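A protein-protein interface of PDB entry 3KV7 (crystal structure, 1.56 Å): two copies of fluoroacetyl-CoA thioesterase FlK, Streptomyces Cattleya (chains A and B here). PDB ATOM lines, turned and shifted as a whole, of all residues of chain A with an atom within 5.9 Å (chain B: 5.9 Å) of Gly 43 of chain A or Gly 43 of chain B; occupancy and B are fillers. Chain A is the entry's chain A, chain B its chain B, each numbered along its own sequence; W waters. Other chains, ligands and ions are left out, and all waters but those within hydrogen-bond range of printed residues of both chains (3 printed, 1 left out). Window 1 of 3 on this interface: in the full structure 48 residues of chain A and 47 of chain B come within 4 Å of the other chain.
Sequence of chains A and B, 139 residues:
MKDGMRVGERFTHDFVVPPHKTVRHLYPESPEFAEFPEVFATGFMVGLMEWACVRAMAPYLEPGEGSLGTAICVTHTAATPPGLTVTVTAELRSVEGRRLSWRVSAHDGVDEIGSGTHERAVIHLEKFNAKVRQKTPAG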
ATOM      1  N   LEU A  26      23.951  30.355  10.812  1.00  0.00           N
ATOM      2  CA  LEU A  26      22.906  29.592  10.047  1.00  0.00           C
ATOM      3  C   LEU A  26      22.451  30.271   8.810  1.00  0.00           C
ATOM      4  O   LEU A  26      22.330  29.685   7.746  1.00  0.00           O
ATOM      5  CB  LEU A  26      21.710  29.272  11.014  1.00  0.00           C
ATOM      6  CG  LEU A  26      20.715  28.221  10.468  1.00  0.00           C
ATOM      7  CD1 LEU A  26      21.281  26.758  10.577  1.00  0.00           C
ATOM      8  CD2 LEU A  26      19.493  28.252  11.357  1.00  0.00           C
ATOM      9  N   TYR A  27      22.261  31.593   8.951  1.00  0.00           N
ATOM     10  CA  TYR A  27      21.909  32.438   7.801  1.00  0.00           C
ATOM     11  C   TYR A  27      22.793  33.716   7.773  1.00  0.00           C
ATOM     12  O   TYR A  27      22.362  34.808   8.297  1.00  0.00           O
ATOM     13  CB  TYR A  27      20.420  32.850   7.832  1.00  0.00           C
ATOM     14  CG  TYR A  27      19.511  31.749   7.280  1.00  0.00           C
ATOM     15  CD1 TYR A  27      19.293  31.671   5.937  1.00  0.00           C
ATOM     16  CD2 TYR A  27      18.970  30.731   8.157  1.00  0.00           C
ATOM     17  CE1 TYR A  27      18.481  30.668   5.374  1.00  0.00           C
ATOM     18  CE2 TYR A  27      18.187  29.697   7.589  1.00  0.00           C
ATOM     19  CZ  TYR A  27      17.933  29.677   6.243  1.00  0.00           C
ATOM     20  OH  TYR A  27      17.221  28.654   5.666  1.00  0.00           O
ATOM     21  N   ALA A  41      22.240  27.819  17.460  1.00  0.00           N
ATOM     22  CA  ALA A  41      20.939  28.104  16.794  1.00  0.00           C
ATOM     23  C   ALA A  41      19.981  26.900  16.923  1.00  0.00           C
ATOM     24  O   ALA A  41      20.384  25.705  16.821  1.00  0.00           O
ATOM     25  CB  ALA A  41      21.191  28.406  15.316  1.00  0.00           C
ATOM     26  N   THR A  42      18.648  27.200  17.026  1.00  0.00           N
ATOM     27  CA  THR A  42      17.680  26.070  17.016  1.00  0.00           C
ATOM     28  C   THR A  42      17.890  25.152  15.790  1.00  0.00           C
ATOM     29  O   THR A  42      17.826  23.943  15.871  1.00  0.00           O
ATOM     30  CB  THR A  42      16.233  26.594  17.097  1.00  0.00           C
ATOM     31  OG1 THR A  42      16.141  27.492  18.222  1.00  0.00           O
ATOM     32  CG2 THR A  42      15.333  25.435  17.185  1.00  0.00           C
ATOM     33  N   GLY A  43      18.082  25.774  14.587  1.00  0.00           N
ATOM     34  CA  GLY A  43      18.206  24.947  13.390  1.00  0.00           C
ATOM     35  C   GLY A  43      19.412  23.999  13.425  1.00  0.00           C
ATOM     36  O   GLY A  43      19.384  22.919  12.909  1.00  0.00           O
ATOM     37  N   PHE A  44      20.488  24.483  14.072  1.00  0.00           N
ATOM     38  CA  PHE A  44      21.638  23.569  14.309  1.00  0.00           C
ATOM     39  C   PHE A  44      21.392  22.513  15.379  1.00  0.00           C
ATOM     40  O   PHE A  44      21.851  21.371  15.199  1.00  0.00           O
ATOM     41  CB  PHE A  44      22.919  24.389  14.619  1.00  0.00           C
ATOM     42  CG  PHE A  44      23.565  25.112  13.443  1.00  0.00           C
ATOM     43  CD1 PHE A  44      23.921  24.428  12.309  1.00  0.00           C
ATOM     44  CD2 PHE A  44      23.849  26.474  13.602  1.00  0.00           C
ATOM     45  CE1 PHE A  44      24.632  25.095  11.220  1.00  0.00           C
ATOM     46  CE2 PHE A  44      24.506  27.153  12.555  1.00  0.00           C
ATOM     47  CZ  PHE A  44      24.870  26.482  11.335  1.00  0.00           C
ATOM     48  N   MET A  45      20.636  22.861  16.449  1.00  0.00           N
ATOM     49  CA  MET A  45      20.199  21.816  17.411  1.00  0.00           C
ATOM     50  C   MET A  45      19.339  20.738  16.701  1.00  0.00           C
ATOM     51  O   MET A  45      19.539  19.536  16.903  1.00  0.00           O
ATOM     52  CB  MET A  45      19.495  22.474  18.590  1.00  0.00           C
ATOM     53  CG  MET A  45      19.129  21.390  19.635  1.00  0.00           C
ATOM     54  SD  MET A  45      18.159  22.024  21.024  1.00  0.00           S
ATOM     55  CE  MET A  45      16.548  22.287  20.188  1.00  0.00           C
ATOM     56  N   VAL A  46      18.429  21.195  15.823  1.00  0.00           N
ATOM     57  CA  VAL A  46      17.640  20.243  15.074  1.00  0.00           C
ATOM     58  C   VAL A  46      18.520  19.328  14.229  1.00  0.00           C
ATOM     59  O   VAL A  46      18.373  18.100  14.202  1.00  0.00           O
ATOM     60  CB  VAL A  46      16.609  20.987  14.221  1.00  0.00           C
ATOM     61  CG1 VAL A  46      15.972  20.034  13.162  1.00  0.00           C
ATOM     62  CG2 VAL A  46      15.537  21.559  15.181  1.00  0.00           C
ATOM     63  N   GLY A  47      19.544  19.956  13.577  1.00  0.00           N
ATOM     64  CA  GLY A  47      20.364  19.142  12.681  1.00  0.00           C
ATOM     65  C   GLY A  47      21.202  18.178  13.542  1.00  0.00           C
ATOM     66  O   GLY A  47      21.390  17.034  13.106  1.00  0.00           O
ATOM     67  N   LEU A  48      21.637  18.592  14.726  1.00  0.00           N
ATOM     68  CA  LEU A  48      22.360  17.646  15.587  1.00  0.00           C
ATOM     69  C   LEU A  48      21.470  16.480  16.094  1.00  0.00           C
ATOM     70  O   LEU A  48      21.944  15.341  16.205  1.00  0.00           O
ATOM     71  CB  LEU A  48      22.990  18.371  16.735  1.00  0.00           C
ATOM     72  CG  LEU A  48      23.875  17.590  17.705  1.00  0.00           C
ATOM     73  CD1 LEU A  48      25.127  17.305  16.950  1.00  0.00           C
ATOM     74  CD2 LEU A  48      24.226  18.496  18.904  1.00  0.00           C
ATOM     75  N   GLU A  50      18.866  15.313  14.458  1.00  0.00           N
ATOM     76  CA  GLU A  50      18.677  14.429  13.293  1.00  0.00           C
ATOM     77  C   GLU A  50      19.958  13.604  13.067  1.00  0.00           C
ATOM     78  O   GLU A  50      19.801  12.411  12.744  1.00  0.00           O
ATOM     79  CB  GLU A  50      18.211  15.255  12.064  1.00  0.00           C
ATOM     80  CG  GLU A  50      16.927  15.927  12.392  1.00  0.00           C
ATOM     81  CD  GLU A  50      16.200  16.720  11.269  1.00  0.00           C
ATOM     82  OE1 GLU A  50      16.791  16.880  10.179  1.00  0.00           O
ATOM     83  OE2 GLU A  50      14.985  17.108  11.532  1.00  0.00           O
ATOM     84  N   LEU B  26      24.798  21.923   6.405  1.00  0.00           N
ATOM     85  CA  LEU B  26      24.398  22.172   7.807  1.00  0.00           C
ATOM     86  C   LEU B  26      25.408  21.674   8.826  1.00  0.00           C
ATOM     87  O   LEU B  26      25.682  22.351   9.841  1.00  0.00           O
ATOM     88  CB  LEU B  26      22.966  21.597   8.022  1.00  0.00           C
ATOM     89  CG  LEU B  26      22.323  21.919   9.387  1.00  0.00           C
ATOM     90  CD1 LEU B  26      21.835  23.360   9.385  1.00  0.00           C
ATOM     91  CD2 LEU B  26      21.104  21.026   9.546  1.00  0.00           C
ATOM     92  N   TYR B  27      25.942  20.502   8.528  1.00  0.00           N
ATOM     93  CA  TYR B  27      27.079  19.960   9.325  1.00  0.00           C
ATOM     94  C   TYR B  27      28.146  19.428   8.414  1.00  0.00           C
ATOM     95  O   TYR B  27      28.142  18.268   8.139  1.00  0.00           O
ATOM     96  CB  TYR B  27      26.599  18.844  10.280  1.00  0.00           C
ATOM     97  CG  TYR B  27      26.049  19.428  11.536  1.00  0.00           C
ATOM     98  CD1 TYR B  27      26.847  19.650  12.675  1.00  0.00           C
ATOM     99  CD2 TYR B  27      24.633  19.764  11.624  1.00  0.00           C
ATOM    100  CE1 TYR B  27      26.345  20.207  13.824  1.00  0.00           C
ATOM    101  CE2 TYR B  27      24.090  20.285  12.804  1.00  0.00           C
ATOM    102  CZ  TYR B  27      24.901  20.532  13.921  1.00  0.00           C
ATOM    103  OH  TYR B  27      24.438  21.107  15.090  1.00  0.00           O
ATOM    104  N   ALA B  41      17.905  21.435   3.894  1.00  0.00           N
ATOM    105  CA  ALA B  41      17.841  20.696   5.188  1.00  0.00           C
ATOM    106  C   ALA B  41      16.760  21.177   6.099  1.00  0.00           C
ATOM    107  O   ALA B  41      16.469  22.406   6.160  1.00  0.00           O
ATOM    108  CB  ALA B  41      19.168  20.855   5.968  1.00  0.00           C
ATOM    109  N   THR B  42      16.175  20.217   6.868  1.00  0.00           N
ATOM    110  CA  THR B  42      15.124  20.646   7.787  1.00  0.00           C
ATOM    111  C   THR B  42      15.639  21.717   8.781  1.00  0.00           C
ATOM    112  O   THR B  42      14.892  22.670   9.097  1.00  0.00           O
ATOM    113  CB  THR B  42      14.636  19.477   8.642  1.00  0.00           C
ATOM    114  OG1 THR B  42      14.225  18.416   7.803  1.00  0.00           O
ATOM    115  CG2 THR B  42      13.515  19.856   9.599  1.00  0.00           C
ATOM    116  N   GLY B  43      16.907  21.606   9.263  1.00  0.00           N
ATOM    117  CA  GLY B  43      17.444  22.631  10.181  1.00  0.00           C
ATOM    118  C   GLY B  43      17.449  24.034   9.516  1.00  0.00           C
ATOM    119  O   GLY B  43      17.231  25.054  10.186  1.00  0.00           O
ATOM    120  N   PHE B  44      17.722  24.062   8.185  1.00  0.00           N
ATOM    121  CA  PHE B  44      17.699  25.365   7.467  1.00  0.00           C
ATOM    122  C   PHE B  44      16.246  25.808   7.269  1.00  0.00           C
ATOM    123  O   PHE B  44      15.963  27.017   7.353  1.00  0.00           O
ATOM    124  CB  PHE B  44      18.424  25.292   6.158  1.00  0.00           C
ATOM    125  CG  PHE B  44      19.943  25.282   6.242  1.00  0.00           C
ATOM    126  CD1 PHE B  44      20.566  26.316   6.910  1.00  0.00           C
ATOM    127  CD2 PHE B  44      20.658  24.241   5.633  1.00  0.00           C
ATOM    128  CE1 PHE B  44      22.040  26.356   6.992  1.00  0.00           C
ATOM    129  CE2 PHE B  44      22.087  24.293   5.644  1.00  0.00           C
ATOM    130  CZ  PHE B  44      22.760  25.294   6.327  1.00  0.00           C
ATOM    131  N   MET B  45      15.309  24.844   7.055  1.00  0.00           N
ATOM    132  CA  MET B  45      13.897  25.273   6.974  1.00  0.00           C
ATOM    133  C   MET B  45      13.386  25.858   8.291  1.00  0.00           C
ATOM    134  O   MET B  45      12.746  26.908   8.273  1.00  0.00           O
ATOM    135  CB  MET B  45      13.026  24.086   6.500  1.00  0.00           C
ATOM    136  CG  MET B  45      11.510  24.556   6.362  1.00  0.00           C
ATOM    137  SD  MET B  45      10.426  23.201   5.918  1.00  0.00           S
ATOM    138  CE  MET B  45      10.371  22.335   7.491  1.00  0.00           C
ATOM    139  N   VAL B  46      13.805  25.286   9.407  1.00  0.00           N
ATOM    140  CA  VAL B  46      13.442  25.789  10.727  1.00  0.00           C
ATOM    141  C   VAL B  46      14.005  27.226  10.852  1.00  0.00           C
ATOM    142  O   VAL B  46      13.288  28.151  11.293  1.00  0.00           O
ATOM    143  CB  VAL B  46      14.030  24.865  11.826  1.00  0.00           C
ATOM    144  CG1 VAL B  46      13.890  25.532  13.230  1.00  0.00           C
ATOM    145  CG2 VAL B  46      13.214  23.522  11.858  1.00  0.00           C
ATOM    146  N   GLY B  47      15.299  27.410  10.500  1.00  0.00           N
ATOM    147  CA  GLY B  47      15.853  28.793  10.624  1.00  0.00           C
ATOM    148  C   GLY B  47      15.116  29.783   9.728  1.00  0.00           C
ATOM    149  O   GLY B  47      14.998  30.978  10.097  1.00  0.00           O
ATOM    150  N   LEU B  48      14.685  29.331   8.550  1.00  0.00           N
ATOM    151  CA  LEU B  48      13.947  30.251   7.647  1.00  0.00           C
ATOM    152  C   LEU B  48      12.591  30.594   8.235  1.00  0.00           C
ATOM    153  O   LEU B  48      12.160  31.731   8.104  1.00  0.00           O
ATOM    154  CB  LEU B  48      13.832  29.523   6.270  1.00  0.00           C
ATOM    155  CG  LEU B  48      13.238  30.431   5.200  1.00  0.00           C
ATOM    156  CD1 LEU B  48      14.292  31.482   4.755  1.00  0.00           C
ATOM    157  CD2 LEU B  48      12.930  29.644   3.984  1.00  0.00           C
ATOM    158  N   GLU B  50      11.955  30.711  11.475  1.00  0.00           N
ATOM    159  CA  GLU B  50      12.266  31.688  12.519  1.00  0.00           C
ATOM    160  C   GLU B  50      12.461  33.082  11.886  1.00  0.00           C
ATOM    161  O   GLU B  50      11.991  34.105  12.418  1.00  0.00           O
ATOM    162  CB  GLU B  50      13.535  31.287  13.307  1.00  0.00           C
ATOM    163  CG  GLU B  50      13.334  30.019  14.125  1.00  0.00           C
ATOM    164  CD  GLU B  50      14.418  29.987  15.170  1.00  0.00           C
ATOM    165  OE1 GLU B  50      14.463  30.823  16.151  1.00  0.00           O
ATOM    166  OE2 GLU B  50      15.289  29.051  15.108  1.00  0.00           O
HETATM  167  O   HOH W   1      12.887  16.452  10.000  1.00  0.00           O
HETATM  168  O   HOH W   2      17.337  28.347  13.811  1.00  0.00           O
HETATM  169  O   HOH W   3      18.296  19.241   9.644  1.00  0.00           O
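The side-chain hydroxyl (OH) of Tyr 27 of chain A sits at hydrogen-bond distance from the backbone carbonyl oxygen (O) of Phe 44 of chain B, 2.7 Å away. The backbone carbonyl oxygen of Phe 44 of chain A is in hydrogen-bond range of the side-chain hydroxyl of Tyr 27 of chain B (2.6 Å).
Among the printed residues, pairs that only touch across the chains: Leu 26 of chain A with Leu 26 of chain B, Leu 26 of chain A with Phe 44 of chain B, Leu 26 of chain A with Gly 47 of chain B, Tyr 27 of chain A with Gly 47 of chain B, Tyr 27 of chain A with Leu 48 of chain B, Thr 42 of chain A with Glu 50 of chain B, Gly 43 of chain A with Gly 43 of chain B, Phe 44 of chain A with Leu 26 of chain B, Gly 47 of chain A with Leu 26 of chain B, Gly 47 of chain A with Tyr 27 of chain B, Leu 48 of chain A with Tyr 27 of chain B and Glu 50 of chain A with Thr 42 of chain B.
Of chain B, only Gly 43 (3.4 Å) comes within 4 Å of Gly 43 of chain A. Of the printed residues of chain A, Gly 43 of chain B touches Gly 43. Of the printed residues of chain A, Leu 26 of chain B touches Leu 26 (3.6 Å), Phe 44 (3.2 Å) and Gly 47 (3.7 Å). Of the printed residues of chain B, Tyr 27 of chain A touches Phe 44 (2.7 Å), Gly 47 (3.7 Å) and Leu 48 (3.6 Å). Printed residues of chain A within 4 Å of Tyr 27 of chain B: Phe 44 (2.6 Å), Gly 47 (3.7 Å) and Leu 48 (3.5 Å). Of the printed residues of chain B, Leu 26 of chain A touches Leu 26 (3.6 Å), Phe 44 (3.4 Å) and Gly 47 (3.8 Å). Of the printed residues of chain B, Leu 48 of chain A touches Tyr 27 (3.5 Å). Met 45 of chain B touches none of the printed residues of chain A.
Hydrophobic or aromatic side chains of chain B that line the printed part of chain A: Leu 26, Tyr 27, Phe 44 and Leu 48. Of the 11 printed residues of chain A, 8 touch a printed residue of chain B. Hydrophobic or aromatic side chains of chain A within 4 Å of the printed part of chain B: Leu 26, Tyr 27, Phe 44 and Leu 48. Along chain A the printed residues that touch a printed residue of chain B span positions 26 to 50. Among the printed residues, 14 pairs touch across the chains.
Leu 26 of chain A touches Gly 47 of chain B, and with the chains exchanged Gly 47 of chain A touches Leu 26 of chain B. Tyr 27 of chain A touches Leu 48 of chain B, and with the chains exchanged Leu 48 of chain A touches Tyr 27 of chain B. Thr 42 of chain A touches Glu 50 of chain B, and with the chains exchanged Glu 50 of chain A touches Thr 42 of chain B. Gly 43 of chain A touches its own counterpart, Gly 43 of chain B. 11 positions are printed for both chains.
Water W2 bridges OE2 of Glu 50 of chain B (2.5 Å) and N of Gly 43 of chain A (2.8 Å). Water W1 bridges OE2 of Glu 50 of chain A (2.7 Å) and OG1 of Thr 42 of chain B (3.2 Å). Water W3 bridges the backbone NH of Gly 43 of chain B and the side-chain carboxylate of Glu 50 of chain A.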
